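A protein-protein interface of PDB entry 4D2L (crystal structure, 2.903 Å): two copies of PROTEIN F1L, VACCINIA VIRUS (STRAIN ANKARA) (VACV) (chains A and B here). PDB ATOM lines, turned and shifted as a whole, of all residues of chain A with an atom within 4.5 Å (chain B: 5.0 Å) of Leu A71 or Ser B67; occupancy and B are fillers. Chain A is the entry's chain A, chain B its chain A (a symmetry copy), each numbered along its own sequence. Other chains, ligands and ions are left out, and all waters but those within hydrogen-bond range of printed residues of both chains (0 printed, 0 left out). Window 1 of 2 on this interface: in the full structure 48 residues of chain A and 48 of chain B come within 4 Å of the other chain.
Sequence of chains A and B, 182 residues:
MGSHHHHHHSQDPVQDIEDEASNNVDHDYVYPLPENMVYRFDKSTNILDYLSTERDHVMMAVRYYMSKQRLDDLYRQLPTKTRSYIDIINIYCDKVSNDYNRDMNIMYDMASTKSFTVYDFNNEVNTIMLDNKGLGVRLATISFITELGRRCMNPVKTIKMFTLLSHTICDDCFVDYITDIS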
ATOM      1  N   SER A  67      16.903  14.701  -2.484  1.00  0.00           N
ATOM      2  CA  SER A  67      15.787  13.968  -3.060  1.00  0.00           C
ATOM      3  C   SER A  67      15.218  14.673  -4.297  1.00  0.00           C
ATOM      4  O   SER A  67      14.906  14.012  -5.283  1.00  0.00           O
ATOM      5  CB  SER A  67      14.707  13.752  -2.000  1.00  0.00           C
ATOM      6  OG  SER A  67      15.073  12.695  -1.116  1.00  0.00           O
ATOM      7  N   LYS A  68      15.103  16.003  -4.267  1.00  0.00           N
ATOM      8  CA  LYS A  68      14.538  16.713  -5.413  1.00  0.00           C
ATOM      9  C   LYS A  68      15.491  16.682  -6.607  1.00  0.00           C
ATOM     10  O   LYS A  68      15.044  16.421  -7.728  1.00  0.00           O
ATOM     11  CB  LYS A  68      14.156  18.168  -5.071  1.00  0.00           C
ATOM     12  CG  LYS A  68      13.072  18.724  -6.031  1.00  0.00           C
ATOM     13  CD  LYS A  68      12.588  20.133  -5.720  1.00  0.00           C
ATOM     14  CE  LYS A  68      11.792  20.698  -6.902  1.00  0.00           C
ATOM     15  NZ  LYS A  68      11.545  22.168  -6.799  1.00  0.00           N
ATOM     16  N   GLN A  69      16.787  16.922  -6.380  1.00  0.00           N
ATOM     17  CA  GLN A  69      17.771  16.796  -7.464  1.00  0.00           C
ATOM     18  C   GLN A  69      17.817  15.380  -8.047  1.00  0.00           C
ATOM     19  O   GLN A  69      17.770  15.241  -9.263  1.00  0.00           O
ATOM     20  CB  GLN A  69      19.179  17.200  -7.014  1.00  0.00           C
ATOM     21  CG  GLN A  69      19.373  18.684  -6.747  1.00  0.00           C
ATOM     22  CD  GLN A  69      19.308  19.538  -7.993  1.00  0.00           C
ATOM     23  OE1 GLN A  69      20.000  19.273  -8.976  1.00  0.00           O
ATOM     24  NE2 GLN A  69      18.465  20.574  -7.960  1.00  0.00           N
ATOM     25  N   ARG A  70      17.894  14.340  -7.211  1.00  0.00           N
ATOM     26  CA  ARG A  70      17.944  12.969  -7.745  1.00  0.00           C
ATOM     27  C   ARG A  70      16.727  12.713  -8.625  1.00  0.00           C
ATOM     28  O   ARG A  70      16.816  12.076  -9.666  1.00  0.00           O
ATOM     29  CB  ARG A  70      18.024  11.911  -6.637  1.00  0.00           C
ATOM     30  CG  ARG A  70      17.734  10.479  -7.119  1.00  0.00           C
ATOM     31  CD  ARG A  70      16.748   9.792  -6.170  1.00  0.00           C
ATOM     32  NE  ARG A  70      16.052   8.627  -6.733  1.00  0.00           N
ATOM     33  CZ  ARG A  70      14.776   8.319  -6.460  1.00  0.00           C
ATOM     34  NH1 ARG A  70      14.065   9.085  -5.624  1.00  0.00           N
ATOM     35  NH2 ARG A  70      14.206   7.243  -7.010  1.00  0.00           N
ATOM     36  N   LEU A  71      15.595  13.270  -8.224  1.00  0.00           N
ATOM     37  CA  LEU A  71      14.333  13.057  -8.923  1.00  0.00           C
ATOM     38  C   LEU A  71      14.222  13.813 -10.248  1.00  0.00           C
ATOM     39  O   LEU A  71      13.763  13.277 -11.256  1.00  0.00           O
ATOM     40  CB  LEU A  71      13.182  13.463  -8.018  1.00  0.00           C
ATOM     41  CG  LEU A  71      11.922  12.616  -8.170  1.00  0.00           C
ATOM     42  CD1 LEU A  71      12.117  11.185  -7.650  1.00  0.00           C
ATOM     43  CD2 LEU A  71      10.796  13.313  -7.460  1.00  0.00           C
ATOM     44  N   ASP A  72      14.608  15.081 -10.239  1.00  0.00           N
ATOM     45  CA  ASP A  72      14.618  15.844 -11.478  1.00  0.00           C
ATOM     46  C   ASP A  72      15.616  15.303 -12.489  1.00  0.00           C
ATOM     47  O   ASP A  72      15.309  15.259 -13.686  1.00  0.00           O
ATOM     48  CB  ASP A  72      14.886  17.335 -11.236  1.00  0.00           C
ATOM     49  CG  ASP A  72      13.930  17.952 -10.269  1.00  0.00           C
ATOM     50  OD1 ASP A  72      12.733  17.603 -10.345  1.00  0.00           O
ATOM     51  OD2 ASP A  72      14.332  18.873  -9.531  1.00  0.00           O
ATOM     52  N   ASP A  73      16.804  14.915 -12.042  1.00  0.00           N
ATOM     53  CA  ASP A  73      17.757  14.371 -12.980  1.00  0.00           C
ATOM     54  C   ASP A  73      17.236  13.070 -13.543  1.00  0.00           C
ATOM     55  O   ASP A  73      17.403  12.772 -14.729  1.00  0.00           O
ATOM     56  CB  ASP A  73      19.102  14.155 -12.326  1.00  0.00           C
ATOM     57  CG  ASP A  73      20.038  13.340 -13.205  1.00  0.00           C
ATOM     58  OD1 ASP A  73      20.024  12.087 -13.107  1.00  0.00           O
ATOM     59  OD2 ASP A  73      20.776  13.946 -14.017  1.00  0.00           O
ATOM     60  N   LEU A  74      16.604  12.299 -12.672  1.00  0.00           N
ATOM     61  CA  LEU A  74      15.996  11.049 -13.078  1.00  0.00           C
ATOM     62  C   LEU A  74      15.024  11.253 -14.224  1.00  0.00           C
ATOM     63  O   LEU A  74      15.055  10.506 -15.198  1.00  0.00           O
ATOM     64  CB  LEU A  74      15.285  10.411 -11.900  1.00  0.00           C
ATOM     65  CG  LEU A  74      14.353   9.245 -12.202  1.00  0.00           C
ATOM     66  CD1 LEU A  74      15.032   8.141 -13.007  1.00  0.00           C
ATOM     67  CD2 LEU A  74      13.841   8.716 -10.883  1.00  0.00           C
ATOM     68  N   TYR A  75      14.160  12.258 -14.116  1.00  0.00           N
ATOM     69  CA  TYR A  75      13.207  12.505 -15.186  1.00  0.00           C
ATOM     70  C   TYR A  75      13.970  12.782 -16.480  1.00  0.00           C
ATOM     71  O   TYR A  75      13.598  12.283 -17.536  1.00  0.00           O
ATOM     72  CB  TYR A  75      12.253  13.662 -14.847  1.00  0.00           C
ATOM     73  CG  TYR A  75      11.282  14.008 -15.969  1.00  0.00           C
ATOM     74  CD1 TYR A  75      10.147  13.235 -16.217  1.00  0.00           C
ATOM     75  CD2 TYR A  75      11.502  15.109 -16.783  1.00  0.00           C
ATOM     76  CE1 TYR A  75       9.262  13.559 -17.257  1.00  0.00           C
ATOM     77  CE2 TYR A  75      10.626  15.437 -17.814  1.00  0.00           C
ATOM     78  CZ  TYR A  75       9.509  14.661 -18.050  1.00  0.00           C
ATOM     79  OH  TYR A  75       8.640  14.989 -19.076  1.00  0.00           O
ATOM     80  N   PHE A 162       6.078   2.662  -1.726  1.00  0.00           N
ATOM     81  CA  PHE A 162       5.980   3.061  -3.114  1.00  0.00           C
ATOM     82  C   PHE A 162       6.470   1.928  -4.018  1.00  0.00           C
ATOM     83  O   PHE A 162       5.785   1.505  -4.960  1.00  0.00           O
ATOM     84  CB  PHE A 162       6.795   4.339  -3.351  1.00  0.00           C
ATOM     85  CG  PHE A 162       6.156   5.580  -2.785  1.00  0.00           C
ATOM     86  CD1 PHE A 162       4.858   5.544  -2.271  1.00  0.00           C
ATOM     87  CD2 PHE A 162       6.830   6.784  -2.791  1.00  0.00           C
ATOM     88  CE1 PHE A 162       4.256   6.682  -1.765  1.00  0.00           C
ATOM     89  CE2 PHE A 162       6.240   7.929  -2.290  1.00  0.00           C
ATOM     90  CZ  PHE A 162       4.950   7.880  -1.773  1.00  0.00           C
ATOM     91  N   ARG B  63       6.084   4.855 -10.062  1.00  0.00           N
ATOM     92  CA  ARG B  63       7.000   5.056  -8.944  1.00  0.00           C
ATOM     93  C   ARG B  63       7.492   6.501  -8.890  1.00  0.00           C
ATOM     94  O   ARG B  63       7.587   7.099  -7.820  1.00  0.00           O
ATOM     95  CB  ARG B  63       8.186   4.093  -9.045  1.00  0.00           C
ATOM     96  CG  ARG B  63       8.610   3.495  -7.707  1.00  0.00           C
ATOM     97  CD  ARG B  63      10.051   2.984  -7.719  1.00  0.00           C
ATOM     98  NE  ARG B  63      10.412   2.328  -8.974  1.00  0.00           N
ATOM     99  CZ  ARG B  63      10.163   1.051  -9.255  1.00  0.00           C
ATOM    100  NH1 ARG B  63       9.541   0.275  -8.374  1.00  0.00           N
ATOM    101  NH2 ARG B  63      10.536   0.555 -10.428  1.00  0.00           N
ATOM    102  N   TYR B  64       7.798   7.054 -10.057  1.00  0.00           N
ATOM    103  CA  TYR B  64       8.199   8.451 -10.169  1.00  0.00           C
ATOM    104  C   TYR B  64       7.079   9.396  -9.710  1.00  0.00           C
ATOM    105  O   TYR B  64       7.350  10.430  -9.090  1.00  0.00           O
ATOM    106  CB  TYR B  64       8.606   8.788 -11.616  1.00  0.00           C
ATOM    107  CG  TYR B  64       8.914  10.259 -11.818  1.00  0.00           C
ATOM    108  CD1 TYR B  64      10.191  10.765 -11.558  1.00  0.00           C
ATOM    109  CD2 TYR B  64       7.933  11.147 -12.248  1.00  0.00           C
ATOM    110  CE1 TYR B  64      10.475  12.115 -11.720  1.00  0.00           C
ATOM    111  CE2 TYR B  64       8.207  12.493 -12.410  1.00  0.00           C
ATOM    112  CZ  TYR B  64       9.479  12.972 -12.148  1.00  0.00           C
ATOM    113  OH  TYR B  64       9.759  14.310 -12.315  1.00  0.00           O
ATOM    114  N   TYR B  65       5.832   9.052 -10.035  1.00  0.00           N
ATOM    115  CA  TYR B  65       4.679   9.887  -9.690  1.00  0.00           C
ATOM    116  C   TYR B  65       4.575  10.043  -8.185  1.00  0.00           C
ATOM    117  O   TYR B  65       4.522  11.171  -7.662  1.00  0.00           O
ATOM    118  CB  TYR B  65       3.375   9.286 -10.246  1.00  0.00           C
ATOM    119  CG  TYR B  65       2.102  10.005  -9.818  1.00  0.00           C
ATOM    120  CD1 TYR B  65       1.720  11.211 -10.402  1.00  0.00           C
ATOM    121  CD2 TYR B  65       1.279   9.474  -8.827  1.00  0.00           C
ATOM    122  CE1 TYR B  65       0.554  11.871 -10.009  1.00  0.00           C
ATOM    123  CE2 TYR B  65       0.110  10.125  -8.428  1.00  0.00           C
ATOM    124  CZ  TYR B  65      -0.250  11.323  -9.024  1.00  0.00           C
ATOM    125  OH  TYR B  65      -1.409  11.963  -8.621  1.00  0.00           O
ATOM    126  N   MET B  66       4.540   8.889  -7.520  1.00  0.00           N
ATOM    127  CA  MET B  66       4.474   8.787  -6.075  1.00  0.00           C
ATOM    128  C   MET B  66       5.571   9.603  -5.386  1.00  0.00           C
ATOM    129  O   MET B  66       5.308  10.422  -4.504  1.00  0.00           O
ATOM    130  CB  MET B  66       4.559   7.311  -5.663  1.00  0.00           C
ATOM    131  CG  MET B  66       3.361   6.440  -6.087  1.00  0.00           C
ATOM    132  SD  MET B  66       3.583   4.672  -5.732  1.00  0.00           S
ATOM    133  CE  MET B  66       1.915   4.018  -5.832  1.00  0.00           C
ATOM    134  N   SER B  67       6.808   9.396  -5.813  1.00  0.00           N
ATOM    135  CA  SER B  67       7.927  10.118  -5.229  1.00  0.00           C
ATOM    136  C   SER B  67       7.814  11.629  -5.456  1.00  0.00           C
ATOM    137  O   SER B  67       8.091  12.403  -4.544  1.00  0.00           O
ATOM    138  CB  SER B  67       9.243   9.571  -5.785  1.00  0.00           C
ATOM    139  OG  SER B  67       9.582   8.336  -5.157  1.00  0.00           O
ATOM    140  N   LYS B  68       7.388  12.058  -6.646  1.00  0.00           N
ATOM    141  CA  LYS B  68       7.293  13.491  -6.916  1.00  0.00           C
ATOM    142  C   LYS B  68       6.153  14.128  -6.122  1.00  0.00           C
ATOM    143  O   LYS B  68       6.353  15.195  -5.533  1.00  0.00           O
ATOM    144  CB  LYS B  68       7.134  13.796  -8.419  1.00  0.00           C
ATOM    145  CG  LYS B  68       7.605  15.231  -8.774  1.00  0.00           C
ATOM    146  CD  LYS B  68       7.544  15.589 -10.252  1.00  0.00           C
ATOM    147  CE  LYS B  68       7.700  17.102 -10.441  1.00  0.00           C
ATOM    148  NZ  LYS B  68       7.353  17.564 -11.820  1.00  0.00           N
ATOM    149  N   GLN B  69       4.981  13.485  -6.082  1.00  0.00           N
ATOM    150  CA  GLN B  69       3.882  13.986  -5.246  1.00  0.00           C
ATOM    151  C   GLN B  69       4.257  14.036  -3.762  1.00  0.00           C
ATOM    152  O   GLN B  69       4.031  15.060  -3.130  1.00  0.00           O
ATOM    153  CB  GLN B  69       2.606  13.155  -5.414  1.00  0.00           C
ATOM    154  CG  GLN B  69       1.910  13.301  -6.758  1.00  0.00           C
ATOM    155  CD  GLN B  69       1.292  14.664  -6.975  1.00  0.00           C
ATOM    156  OE1 GLN B  69       0.531  15.153  -6.140  1.00  0.00           O
ATOM    157  NE2 GLN B  69       1.623  15.293  -8.107  1.00  0.00           N
ATOM    158  N   ARG B  70       4.829  12.964  -3.204  1.00  0.00           N
ATOM    159  CA  ARG B  70       5.196  12.985  -1.777  1.00  0.00           C
ATOM    160  C   ARG B  70       6.131  14.155  -1.502  1.00  0.00           C
ATOM    161  O   ARG B  70       6.032  14.822  -0.480  1.00  0.00           O
ATOM    162  CB  ARG B  70       5.845  11.672  -1.321  1.00  0.00           C
ATOM    163  CG  ARG B  70       6.547  11.765   0.045  1.00  0.00           C
ATOM    164  CD  ARG B  70       7.940  11.133  -0.032  1.00  0.00           C
ATOM    165  NE  ARG B  70       8.868  11.540   1.030  1.00  0.00           N
ATOM    166  CZ  ARG B  70      10.182  11.724   0.839  1.00  0.00           C
ATOM    167  NH1 ARG B  70      10.719  11.525  -0.370  1.00  0.00           N
ATOM    168  NH2 ARG B  70      10.968  12.097   1.853  1.00  0.00           N
ATOM    169  N   LEU B  71       7.006  14.435  -2.454  1.00  0.00           N
ATOM    170  CA  LEU B  71       8.011  15.480  -2.305  1.00  0.00           C
ATOM    171  C   LEU B  71       7.452  16.900  -2.417  1.00  0.00           C
ATOM    172  O   LEU B  71       7.802  17.789  -1.642  1.00  0.00           O
ATOM    173  CB  LEU B  71       9.096  15.287  -3.351  1.00  0.00           C
ATOM    174  CG  LEU B  71      10.501  15.665  -2.889  1.00  0.00           C
ATOM    175  CD1 LEU B  71      11.044  14.700  -1.827  1.00  0.00           C
ATOM    176  CD2 LEU B  71      11.396  15.719  -4.094  1.00  0.00           C
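Leu A71 touches just these residues of chain B: Tyr B64 (3.5 Å), Ser B67 (3.8 Å) and Lys B68 (3.5 Å). Of the printed residues of chain B, Tyr A75 touches Tyr B64 (3.6 Å). Of the printed residues of chain A, Met B66 touches Phe A162. Ser B67 touches just these residues of chain A: Leu A71 and Phe A162. Gln B69 touches none of the printed residues of chain A. Of the printed residues of chain A, Arg B70 touches Phe A162. The nearest printed residue of chain B that does not touch Lys A68 is Lys B68 (6.5 Å).
Leu B71 touches Ser A67 (CD1 to CB, 3.8 Å). CD2 of Leu B71 touches CA of Lys A68, at 3.5 Å. Leu A71 touches Tyr B64 (O to CE1, 3.5 Å). CD1 of Leu A71 touches CB of Ser B67 (3.8 Å). Leu A71 touches Lys B68 (CD2 to CA, 3.5 Å). CB of Tyr A75 touches OH of Tyr B64 (3.6 Å). Phe A162 touches Met B66 (CE2 to O, 3.5 Å). Ser B67 touches Phe A162. CB of Arg B70 touches CE2 of Phe A162, at 3.9 Å.
Ser A67 touches Leu B71, and with the chains exchanged Leu A71 touches Ser B67. Lys A68 touches Leu B71, and with the chains exchanged Leu A71 touches Lys B68. Of the 9 pairs that touch across the chains among the printed residues, 4 have their exchanged pair printed and touching as well.
Hydrophobic or aromatic side chains of chain B that line the printed part of chain A: Tyr B64, Met B66 and Leu B71. Among the printed residues, no Asp or Glu carboxylate lies within 4 Å of a Lys or Arg side-chain nitrogen of the other chain.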
